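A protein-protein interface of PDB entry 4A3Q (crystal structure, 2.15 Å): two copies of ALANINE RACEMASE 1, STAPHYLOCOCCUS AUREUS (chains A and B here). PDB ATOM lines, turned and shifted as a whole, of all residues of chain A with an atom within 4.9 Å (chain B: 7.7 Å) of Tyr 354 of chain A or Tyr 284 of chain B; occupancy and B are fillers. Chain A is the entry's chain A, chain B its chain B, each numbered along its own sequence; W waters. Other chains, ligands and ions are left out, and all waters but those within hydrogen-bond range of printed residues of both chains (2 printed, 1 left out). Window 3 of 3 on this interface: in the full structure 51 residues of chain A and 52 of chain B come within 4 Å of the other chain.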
ATOM      1  N   TYR A  43      13.482   7.050 -22.426  1.00  0.00           N
ATOM      2  CA  TYR A  43      13.451   8.459 -21.995  1.00  0.00           C
ATOM      3  C   TYR A  43      12.834   9.327 -23.087  1.00  0.00           C
ATOM      4  O   TYR A  43      13.246  10.475 -23.301  1.00  0.00           O
ATOM      5  CB  TYR A  43      14.858   8.963 -21.648  1.00  0.00           C
ATOM      6  CG  TYR A  43      15.504   8.282 -20.444  1.00  0.00           C
ATOM      7  CD1 TYR A  43      15.436   6.899 -20.279  1.00  0.00           C
ATOM      8  CD2 TYR A  43      16.212   9.027 -19.486  1.00  0.00           C
ATOM      9  CE1 TYR A  43      16.040   6.273 -19.188  1.00  0.00           C
ATOM     10  CE2 TYR A  43      16.797   8.419 -18.393  1.00  0.00           C
ATOM     11  CZ  TYR A  43      16.720   7.046 -18.245  1.00  0.00           C
ATOM     12  OH  TYR A  43      17.321   6.418 -17.182  1.00  0.00           O
ATOM     13  N   ILE A 222      20.239   7.981 -18.910  1.00  0.00           N
ATOM     14  CA  ILE A 222      20.127   9.266 -19.583  1.00  0.00           C
ATOM     15  C   ILE A 222      21.349   9.619 -20.450  1.00  0.00           C
ATOM     16  O   ILE A 222      21.179  10.256 -21.475  1.00  0.00           O
ATOM     17  CB  ILE A 222      19.814  10.431 -18.604  1.00  0.00           C
ATOM     18  CG1 ILE A 222      19.389  11.671 -19.411  1.00  0.00           C
ATOM     19  CG2 ILE A 222      21.020  10.686 -17.662  1.00  0.00           C
ATOM     20  CD1 ILE A 222      18.884  12.831 -18.585  1.00  0.00           C
ATOM     21  N   PRO A 229      23.598  13.670 -16.122  1.00  0.00           N
ATOM     22  CA  PRO A 229      22.658  13.675 -15.005  1.00  0.00           C
ATOM     23  C   PRO A 229      22.688  14.960 -14.164  1.00  0.00           C
ATOM     24  O   PRO A 229      21.681  15.268 -13.489  1.00  0.00           O
ATOM     25  CB  PRO A 229      23.085  12.464 -14.161  1.00  0.00           C
ATOM     26  CG  PRO A 229      24.435  12.095 -14.625  1.00  0.00           C
ATOM     27  CD  PRO A 229      24.589  12.583 -16.038  1.00  0.00           C
ATOM     28  N   ILE A 352      14.269  19.001 -14.295  1.00  0.00           N
ATOM     29  CA  ILE A 352      15.530  18.429 -14.753  1.00  0.00           C
ATOM     30  C   ILE A 352      15.398  17.893 -16.169  1.00  0.00           C
ATOM     31  O   ILE A 352      14.287  17.565 -16.613  1.00  0.00           O
ATOM     32  CB  ILE A 352      16.042  17.312 -13.786  1.00  0.00           C
ATOM     33  CG1 ILE A 352      15.035  16.146 -13.643  1.00  0.00           C
ATOM     34  CG2 ILE A 352      16.413  17.932 -12.448  1.00  0.00           C
ATOM     35  CD1 ILE A 352      15.478  15.035 -12.668  1.00  0.00           C
ATOM     36  N   ASN A 353      16.525  17.792 -16.866  1.00  0.00           N
ATOM     37  CA  ASN A 353      16.530  17.327 -18.249  1.00  0.00           C
ATOM     38  C   ASN A 353      15.728  16.044 -18.465  1.00  0.00           C
ATOM     39  O   ASN A 353      15.012  15.956 -19.445  1.00  0.00           O
ATOM     40  CB  ASN A 353      17.958  17.230 -18.825  1.00  0.00           C
ATOM     41  CG  ASN A 353      18.916  16.443 -17.927  1.00  0.00           C
ATOM     42  OD1 ASN A 353      18.486  15.734 -17.010  1.00  0.00           O
ATOM     43  ND2 ASN A 353      20.232  16.557 -18.201  1.00  0.00           N
ATOM     44  N   TYR A 354      15.808  15.086 -17.530  1.00  0.00           N
ATOM     45  CA  TYR A 354      15.079  13.809 -17.619  1.00  0.00           C
ATOM     46  C   TYR A 354      13.596  14.046 -17.921  1.00  0.00           C
ATOM     47  O   TYR A 354      13.024  13.381 -18.760  1.00  0.00           O
ATOM     48  CB  TYR A 354      15.131  13.042 -16.292  1.00  0.00           C
ATOM     49  CG  TYR A 354      16.483  12.511 -15.798  1.00  0.00           C
ATOM     50  CD1 TYR A 354      17.395  13.356 -15.160  1.00  0.00           C
ATOM     51  CD2 TYR A 354      16.806  11.146 -15.896  1.00  0.00           C
ATOM     52  CE1 TYR A 354      18.612  12.875 -14.670  1.00  0.00           C
ATOM     53  CE2 TYR A 354      18.026  10.650 -15.390  1.00  0.00           C
ATOM     54  CZ  TYR A 354      18.922  11.527 -14.794  1.00  0.00           C
ATOM     55  OH  TYR A 354      20.123  11.077 -14.298  1.00  0.00           O
ATOM     56  N   GLU A 355      12.985  14.970 -17.195  1.00  0.00           N
ATOM     57  CA  GLU A 355      11.549  15.216 -17.284  1.00  0.00           C
ATOM     58  C   GLU A 355      11.176  15.933 -18.577  1.00  0.00           C
ATOM     59  O   GLU A 355      10.111  15.669 -19.162  1.00  0.00           O
ATOM     60  CB  GLU A 355      11.039  16.008 -16.068  1.00  0.00           C
ATOM     61  CG  GLU A 355       9.518  16.039 -15.954  1.00  0.00           C
ATOM     62  CD  GLU A 355       9.028  16.704 -14.687  1.00  0.00           C
ATOM     63  OE1 GLU A 355       9.119  17.946 -14.552  1.00  0.00           O
ATOM     64  OE2 GLU A 355       8.529  15.979 -13.819  1.00  0.00           O
ATOM     65  N   VAL A 356      12.049  16.828 -19.035  1.00  0.00           N
ATOM     66  CA  VAL A 356      11.777  17.515 -20.279  1.00  0.00           C
ATOM     67  C   VAL A 356      11.586  16.461 -21.377  1.00  0.00           C
ATOM     68  O   VAL A 356      10.670  16.567 -22.172  1.00  0.00           O
ATOM     69  CB  VAL A 356      12.915  18.467 -20.669  1.00  0.00           C
ATOM     70  CG1 VAL A 356      12.794  18.928 -22.143  1.00  0.00           C
ATOM     71  CG2 VAL A 356      12.970  19.681 -19.704  1.00  0.00           C
ATOM     72  N   LEU A 357      12.466  15.460 -21.395  1.00  0.00           N
ATOM     73  CA  LEU A 357      12.429  14.401 -22.399  1.00  0.00           C
ATOM     74  C   LEU A 357      11.175  13.561 -22.257  1.00  0.00           C
ATOM     75  O   LEU A 357      10.501  13.275 -23.254  1.00  0.00           O
ATOM     76  CB  LEU A 357      13.661  13.493 -22.301  1.00  0.00           C
ATOM     77  CG  LEU A 357      15.013  14.130 -22.639  1.00  0.00           C
ATOM     78  CD1 LEU A 357      16.139  13.242 -22.167  1.00  0.00           C
ATOM     79  CD2 LEU A 357      15.132  14.390 -24.117  1.00  0.00           C
ATOM     80  N   CYS A 358      10.901  13.148 -21.019  1.00  0.00           N
ATOM     81  CA  CYS A 358       9.755  12.290 -20.707  1.00  0.00           C
ATOM     82  C   CYS A 358       8.442  12.948 -21.069  1.00  0.00           C
ATOM     83  O   CYS A 358       7.498  12.251 -21.394  1.00  0.00           O
ATOM     84  CB  CYS A 358       9.743  11.927 -19.221  1.00  0.00           C
ATOM     85  SG  CYS A 358      10.975  10.708 -18.890  1.00  0.00           S
ATOM     86  N   ILE B 282       4.816   4.559  -9.851  1.00  0.00           N
ATOM     87  CA  ILE B 282       4.375   5.600 -10.762  1.00  0.00           C
ATOM     88  C   ILE B 282       5.294   6.827 -10.567  1.00  0.00           C
ATOM     89  O   ILE B 282       5.741   7.114  -9.446  1.00  0.00           O
ATOM     90  CB  ILE B 282       2.858   5.958 -10.546  1.00  0.00           C
ATOM     91  CG1 ILE B 282       2.317   6.831 -11.684  1.00  0.00           C
ATOM     92  CG2 ILE B 282       2.627   6.634  -9.184  1.00  0.00           C
ATOM     93  CD1 ILE B 282       0.794   7.166 -11.523  1.00  0.00           C
ATOM     94  N   GLY B 283       5.594   7.537 -11.650  1.00  0.00           N
ATOM     95  CA  GLY B 283       6.519   8.672 -11.534  1.00  0.00           C
ATOM     96  C   GLY B 283       6.309   9.685 -12.624  1.00  0.00           C
ATOM     97  O   GLY B 283       5.268   9.654 -13.310  1.00  0.00           O
ATOM     98  N   TYR B 284       7.286  10.579 -12.798  1.00  0.00           N
ATOM     99  CA  TYR B 284       7.098  11.675 -13.719  1.00  0.00           C
ATOM    100  C   TYR B 284       7.017  11.257 -15.183  1.00  0.00           C
ATOM    101  O   TYR B 284       6.422  11.971 -15.961  1.00  0.00           O
ATOM    102  CB  TYR B 284       8.092  12.847 -13.498  1.00  0.00           C
ATOM    103  CG  TYR B 284       9.589  12.536 -13.619  1.00  0.00           C
ATOM    104  CD1 TYR B 284      10.188  12.432 -14.861  1.00  0.00           C
ATOM    105  CD2 TYR B 284      10.392  12.367 -12.472  1.00  0.00           C
ATOM    106  CE1 TYR B 284      11.554  12.164 -14.983  1.00  0.00           C
ATOM    107  CE2 TYR B 284      11.757  12.096 -12.576  1.00  0.00           C
ATOM    108  CZ  TYR B 284      12.322  12.012 -13.833  1.00  0.00           C
ATOM    109  OH  TYR B 284      13.651  11.739 -13.982  1.00  0.00           O
ATOM    110  N   ALA B 285       7.609  10.117 -15.549  1.00  0.00           N
ATOM    111  CA  ALA B 285       7.431   9.534 -16.915  1.00  0.00           C
ATOM    112  C   ALA B 285       5.995   9.122 -17.220  1.00  0.00           C
ATOM    113  O   ALA B 285       5.636   8.979 -18.397  1.00  0.00           O
ATOM    114  CB  ALA B 285       8.348   8.328 -17.120  1.00  0.00           C
ATOM    115  N   ASP B 286       5.193   8.902 -16.177  1.00  0.00           N
ATOM    116  CA  ASP B 286       3.763   8.663 -16.346  1.00  0.00           C
ATOM    117  C   ASP B 286       2.946   9.947 -16.368  1.00  0.00           C
ATOM    118  O   ASP B 286       1.742   9.905 -16.583  1.00  0.00           O
ATOM    119  CB  ASP B 286       3.260   7.732 -15.239  1.00  0.00           C
ATOM    120  CG  ASP B 286       3.994   6.431 -15.228  1.00  0.00           C
ATOM    121  OD1 ASP B 286       3.853   5.642 -16.194  1.00  0.00           O
ATOM    122  OD2 ASP B 286       4.760   6.216 -14.288  1.00  0.00           O
ATOM    123  N   GLY B 287       3.612  11.078 -16.123  1.00  0.00           N
ATOM    124  CA  GLY B 287       2.958  12.382 -16.053  1.00  0.00           C
ATOM    125  C   GLY B 287       2.662  12.886 -14.647  1.00  0.00           C
ATOM    126  O   GLY B 287       2.034  13.933 -14.485  1.00  0.00           O
ATOM    127  N   TYR B 288       3.090  12.139 -13.628  1.00  0.00           N
ATOM    128  CA  TYR B 288       3.014  12.608 -12.238  1.00  0.00           C
ATOM    129  C   TYR B 288       4.289  13.382 -11.959  1.00  0.00           C
ATOM    130  O   TYR B 288       5.288  12.817 -11.511  1.00  0.00           O
ATOM    131  CB  TYR B 288       2.846  11.433 -11.269  1.00  0.00           C
ATOM    132  CG  TYR B 288       2.275  11.864  -9.943  1.00  0.00           C
ATOM    133  CD1 TYR B 288       0.937  12.243  -9.829  1.00  0.00           C
ATOM    134  CD2 TYR B 288       3.087  11.947  -8.808  1.00  0.00           C
ATOM    135  CE1 TYR B 288       0.409  12.683  -8.598  1.00  0.00           C
ATOM    136  CE2 TYR B 288       2.567  12.383  -7.562  1.00  0.00           C
ATOM    137  CZ  TYR B 288       1.236  12.739  -7.469  1.00  0.00           C
ATOM    138  OH  TYR B 288       0.742  13.149  -6.261  1.00  0.00           O
ATOM    139  N   LEU B 289       4.250  14.680 -12.257  1.00  0.00           N
ATOM    140  CA  LEU B 289       5.458  15.472 -12.409  1.00  0.00           C
ATOM    141  C   LEU B 289       6.205  15.716 -11.076  1.00  0.00           C
ATOM    142  O   LEU B 289       5.636  15.599  -9.988  1.00  0.00           O
ATOM    143  CB  LEU B 289       5.152  16.772 -13.167  1.00  0.00           C
ATOM    144  CG  LEU B 289       4.532  16.700 -14.582  1.00  0.00           C
ATOM    145  CD1 LEU B 289       4.518  18.087 -15.239  1.00  0.00           C
ATOM    146  CD2 LEU B 289       5.195  15.686 -15.529  1.00  0.00           C
ATOM    147  N   ARG B 290       7.493  15.977 -11.161  1.00  0.00           N
ATOM    148  CA  ARG B 290       8.331  16.128  -9.957  1.00  0.00           C
ATOM    149  C   ARG B 290       7.770  17.169  -8.980  1.00  0.00           C
ATOM    150  O   ARG B 290       7.868  17.001  -7.774  1.00  0.00           O
ATOM    151  CB  ARG B 290       9.740  16.516 -10.357  1.00  0.00           C
ATOM    152  CG  ARG B 290      10.444  15.434 -11.174  1.00  0.00           C
ATOM    153  CD  ARG B 290      11.784  15.917 -11.706  1.00  0.00           C
ATOM    154  NE  ARG B 290      12.803  16.122 -10.676  1.00  0.00           N
ATOM    155  CZ  ARG B 290      13.250  17.308 -10.252  1.00  0.00           C
ATOM    156  NH1 ARG B 290      12.750  18.448 -10.734  1.00  0.00           N
ATOM    157  NH2 ARG B 290      14.204  17.353  -9.328  1.00  0.00           N
ATOM    158  N   ILE B 291       7.180  18.232  -9.526  1.00  0.00           N
ATOM    159  CA  ILE B 291       6.575  19.308  -8.740  1.00  0.00           C
ATOM    160  C   ILE B 291       5.460  18.773  -7.827  1.00  0.00           C
ATOM    161  O   ILE B 291       4.977  19.513  -6.973  1.00  0.00           O
ATOM    162  CB  ILE B 291       6.022  20.440  -9.678  1.00  0.00           C
ATOM    163  CG1 ILE B 291       5.641  21.721  -8.887  1.00  0.00           C
ATOM    164  CG2 ILE B 291       4.839  19.916 -10.517  1.00  0.00           C
ATOM    165  CD1 ILE B 291       5.591  22.998  -9.732  1.00  0.00           C
ATOM    166  N   ARG B 309      11.975  13.229  -3.470  1.00  0.00           N
ATOM    167  CA  ARG B 309      11.796  13.467  -4.897  1.00  0.00           C
ATOM    168  C   ARG B 309      10.868  12.447  -5.566  1.00  0.00           C
ATOM    169  O   ARG B 309      10.918  11.244  -5.285  1.00  0.00           O
ATOM    170  CB  ARG B 309      13.149  13.489  -5.604  1.00  0.00           C
ATOM    171  CG  ARG B 309      14.113  14.540  -5.069  1.00  0.00           C
ATOM    172  CD  ARG B 309      13.726  15.946  -5.492  1.00  0.00           C
ATOM    173  NE  ARG B 309      14.845  16.864  -5.300  1.00  0.00           N
ATOM    174  CZ  ARG B 309      14.770  18.195  -5.365  1.00  0.00           C
ATOM    175  NH1 ARG B 309      13.614  18.805  -5.614  1.00  0.00           N
ATOM    176  NH2 ARG B 309      15.866  18.922  -5.172  1.00  0.00           N
ATOM    177  N   VAL B 310      10.007  12.941  -6.439  1.00  0.00           N
ATOM    178  CA  VAL B 310       9.246  12.052  -7.327  1.00  0.00           C
ATOM    179  C   VAL B 310      10.250  11.605  -8.354  1.00  0.00           C
ATOM    180  O   VAL B 310      10.937  12.447  -8.935  1.00  0.00           O
ATOM    181  CB  VAL B 310       8.070  12.801  -8.034  1.00  0.00           C
ATOM    182  CG1 VAL B 310       7.442  11.938  -9.119  1.00  0.00           C
ATOM    183  CG2 VAL B 310       7.015  13.244  -7.011  1.00  0.00           C
ATOM    184  N   CYS B 311      10.363  10.299  -8.552  1.00  0.00           N
ATOM    185  CA  CYS B 311      11.299   9.742  -9.532  1.00  0.00           C
ATOM    186  C   CYS B 311      10.604   9.445 -10.855  1.00  0.00           C
ATOM    187  O   CYS B 311       9.411   9.706 -11.002  1.00  0.00           O
ATOM    188  CB  CYS B 311      11.986   8.500  -8.953  1.00  0.00           C
ATOM    189  SG  CYS B 311      13.122   9.049  -7.650  1.00  0.00           S
ATOM    190  N   MET B 312      11.355   8.933 -11.826  1.00  0.00           N
ATOM    191  CA  MET B 312      10.822   8.713 -13.180  1.00  0.00           C
ATOM    192  C   MET B 312       9.695   7.679 -13.123  1.00  0.00           C
ATOM    193  O   MET B 312       8.681   7.848 -13.787  1.00  0.00           O
ATOM    194  CB  MET B 312      11.940   8.250 -14.136  1.00  0.00           C
ATOM    195  CG  MET B 312      11.493   7.967 -15.589  1.00  0.00           C
ATOM    196  SD  MET B 312      12.859   7.699 -16.815  1.00  0.00           S
ATOM    197  CE  MET B 312      13.916   9.014 -16.287  1.00  0.00           C
ATOM    198  N   ASP B 313       9.895   6.652 -12.301  1.00  0.00           N
ATOM    199  CA  ASP B 313       9.030   5.460 -12.229  1.00  0.00           C
ATOM    200  C   ASP B 313       8.516   5.157 -10.793  1.00  0.00           C
ATOM    201  O   ASP B 313       7.903   4.135 -10.556  1.00  0.00           O
ATOM    202  CB  ASP B 313       9.804   4.236 -12.750  1.00  0.00           C
ATOM    203  CG  ASP B 313      10.545   4.510 -14.057  1.00  0.00           C
ATOM    204  OD1 ASP B 313       9.928   4.908 -15.078  1.00  0.00           O
ATOM    205  OD2 ASP B 313      11.758   4.262 -14.086  1.00  0.00           O
ATOM    206  N   GLN B 314       8.784   6.035  -9.837  1.00  0.00           N
ATOM    207  CA  GLN B 314       8.492   5.737  -8.449  1.00  0.00           C
ATOM    208  C   GLN B 314       8.188   6.984  -7.663  1.00  0.00           C
ATOM    209  O   GLN B 314       8.883   8.016  -7.809  1.00  0.00           O
ATOM    210  CB  GLN B 314       9.683   5.025  -7.821  1.00  0.00           C
ATOM    211  CG  GLN B 314       9.546   4.682  -6.343  1.00  0.00           C
ATOM    212  CD  GLN B 314      10.744   3.882  -5.910  1.00  0.00           C
ATOM    213  OE1 GLN B 314      10.693   2.578  -6.173  1.00  0.00           O
ATOM    214  NE2 GLN B 314      11.754   4.441  -5.437  1.00  0.00           N
ATOM    215  N   THR B 315       7.175   6.866  -6.804  1.00  0.00           N
ATOM    216  CA  THR B 315       6.767   7.936  -5.900  1.00  0.00           C
ATOM    217  C   THR B 315       6.723   7.433  -4.455  1.00  0.00           C
ATOM    218  O   THR B 315       6.291   6.305  -4.192  1.00  0.00           O
ATOM    219  CB  THR B 315       5.377   8.489  -6.296  1.00  0.00           C
ATOM    220  OG1 THR B 315       5.420   8.890  -7.669  1.00  0.00           O
ATOM    221  CG2 THR B 315       5.024   9.718  -5.441  1.00  0.00           C
ATOM    222  N   ASN B 359      -0.837  15.659 -19.589  1.00  0.00           N
ATOM    223  CA  ASN B 359       0.443  15.143 -19.053  1.00  0.00           C
ATOM    224  C   ASN B 359       0.459  13.637 -18.852  1.00  0.00           C
ATOM    225  O   ASN B 359       1.536  13.037 -18.807  1.00  0.00           O
ATOM    226  CB  ASN B 359       0.747  15.763 -17.688  1.00  0.00           C
ATOM    227  CG  ASN B 359       1.360  17.161 -17.774  1.00  0.00           C
ATOM    228  OD1 ASN B 359       1.788  17.607 -18.834  1.00  0.00           O
ATOM    229  ND2 ASN B 359       1.407  17.856 -16.624  1.00  0.00           N
ATOM    230  N   LEU B 360      -0.726  13.039 -18.697  1.00  0.00           N
ATOM    231  CA  LEU B 360      -0.806  11.625 -18.343  1.00  0.00           C
ATOM    232  C   LEU B 360      -0.311  10.822 -19.524  1.00  0.00           C
ATOM    233  O   LEU B 360      -0.825  10.969 -20.641  1.00  0.00           O
ATOM    234  CB  LEU B 360      -2.237  11.246 -17.960  1.00  0.00           C
ATOM    235  CG  LEU B 360      -2.756  12.101 -16.783  1.00  0.00           C
ATOM    236  CD1 LEU B 360      -4.191  11.754 -16.434  1.00  0.00           C
ATOM    237  CD2 LEU B 360      -1.833  11.986 -15.561  1.00  0.00           C
ATOM    238  N   SER B 361       0.712  10.008 -19.300  1.00  0.00           N
ATOM    239  CA  SER B 361       1.488   9.493 -20.424  1.00  0.00           C
ATOM    240  C   SER B 361       0.975   8.171 -21.019  1.00  0.00           C
ATOM    241  O   SER B 361       0.115   7.507 -20.439  1.00  0.00           O
ATOM    242  CB  SER B 361       2.963   9.368 -20.033  1.00  0.00           C
ATOM    243  OG  SER B 361       3.301   8.021 -19.759  1.00  0.00           O
ATOM    244  N   ARG B 363       2.250   5.364 -21.099  1.00  0.00           N
ATOM    245  CA  ARG B 363       2.609   4.198 -20.326  1.00  0.00           C
ATOM    246  C   ARG B 363       1.468   3.721 -19.423  1.00  0.00           C
ATOM    247  O   ARG B 363       1.439   2.547 -19.050  1.00  0.00           O
ATOM    248  CB  ARG B 363       3.887   4.465 -19.507  1.00  0.00           C
ATOM    249  CG  ARG B 363       4.486   3.187 -18.906  1.00  0.00           C
ATOM    250  CD  ARG B 363       5.914   3.367 -18.446  1.00  0.00           C
ATOM    251  NE  ARG B 363       6.024   4.258 -17.291  1.00  0.00           N
ATOM    252  CZ  ARG B 363       7.161   4.489 -16.652  1.00  0.00           C
ATOM    253  NH1 ARG B 363       8.280   3.888 -17.076  1.00  0.00           N
ATOM    254  NH2 ARG B 363       7.182   5.304 -15.596  1.00  0.00           N
HETATM  255  O   HOH W   1       8.058  19.313 -12.395  1.00  0.00           O
HETATM  256  O   HOH W   2       6.408  13.263 -18.278  1.00  0.00           O
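OE2 of Glu 355 of chain A sits at hydrogen-bond distance from N of Arg 290 of chain B, 2.9 Å away.
O of Tyr 354 of chain A sits at hydrogen-bond distance from SG of Cys 358 of chain A (3.4 Å).
The backbone NH of Tyr 284 of chain B is in hydrogen-bond range of the backbone carbonyl oxygen of Cys 311 of chain B.
The backbone NH (N) of Tyr 284 of chain B lies within hydrogen-bond range of the backbone carbonyl oxygen (O) of Met 312 of chain B, at 3.2 Å.
The backbone carbonyl oxygen (O) of Met 312 of chain B is in hydrogen-bond range of the backbone NH (N) of Ala 285 of chain B (3.1 Å).
The backbone carbonyl oxygen (O) of Ala 285 of chain B is in hydrogen-bond range of the side-chain hydroxyl (OG) of Ser 361 of chain B, 2.9 Å away.
NH2 of Arg 363 of chain B sits at hydrogen-bond distance from O of Met 312 of chain B.
Among the printed residues, merely in contact across the chains: Tyr 354 of chain A with Tyr 284 of chain B, Glu 355 of chain A with Tyr 284 of chain B, Glu 355 of chain A with Leu 289 of chain B, Ile 352 of chain A with Arg 290 of chain B, Tyr 354 of chain A with Met 312 of chain B, Tyr 43 of chain A with Met 312 of chain B, Cys 358 of chain A with Ala 285 of chain B and Ile 352 of chain A with Tyr 284 of chain B.
Of the printed residues of chain B, Ile 352 of chain A touches Tyr 284 (3.99 Å) and Arg 290 (3.5 Å).
Printed residues of chain A within 4 Å of Tyr 284 of chain B: Ile 352, Tyr 354 and Glu 355.
Of the printed residues of chain A, Ala 285 of chain B touches Cys 358 (3.96 Å).
Tyr 288 of chain B touches none of the printed residues of chain A.
The nearest printed residue of chain A that does not touch Tyr 284 of chain B is Cys 358 of chain A (4.2 Å).
Of the 21 printed residues of chain B, 5 touch a printed residue of chain A.
Printed residues of chain B that touch a printed residue of chain A: Tyr 284, Ala 285, Leu 289, Arg 290 and Met 312.
Hydrophobic or aromatic side chains of chain B that line the printed part of chain A: Tyr 284, Ala 285, Leu 289 and Met 312.
Hydrophobic or aromatic side chains of chain A that line the printed part of chain B: Tyr 43, Ile 352 and Tyr 354.
Along chain A the printed residues that touch a printed residue of chain B span positions 43 to 358.
No position is printed for both chains.
Of the 9 pairs that touch across the chains among the printed residues, none has its exchanged pair printed and touching as well.
Water W2 lies within hydrogen-bond range of the backbone carbonyl oxygen of Tyr 284 of chain B and the backbone carbonyl oxygen of Cys 358 of chain A.
Water W1 lies within hydrogen-bond range of OE1 of Glu 355 of chain A (2.8 Å) and N of Ile 291 of chain B (3.2 Å).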
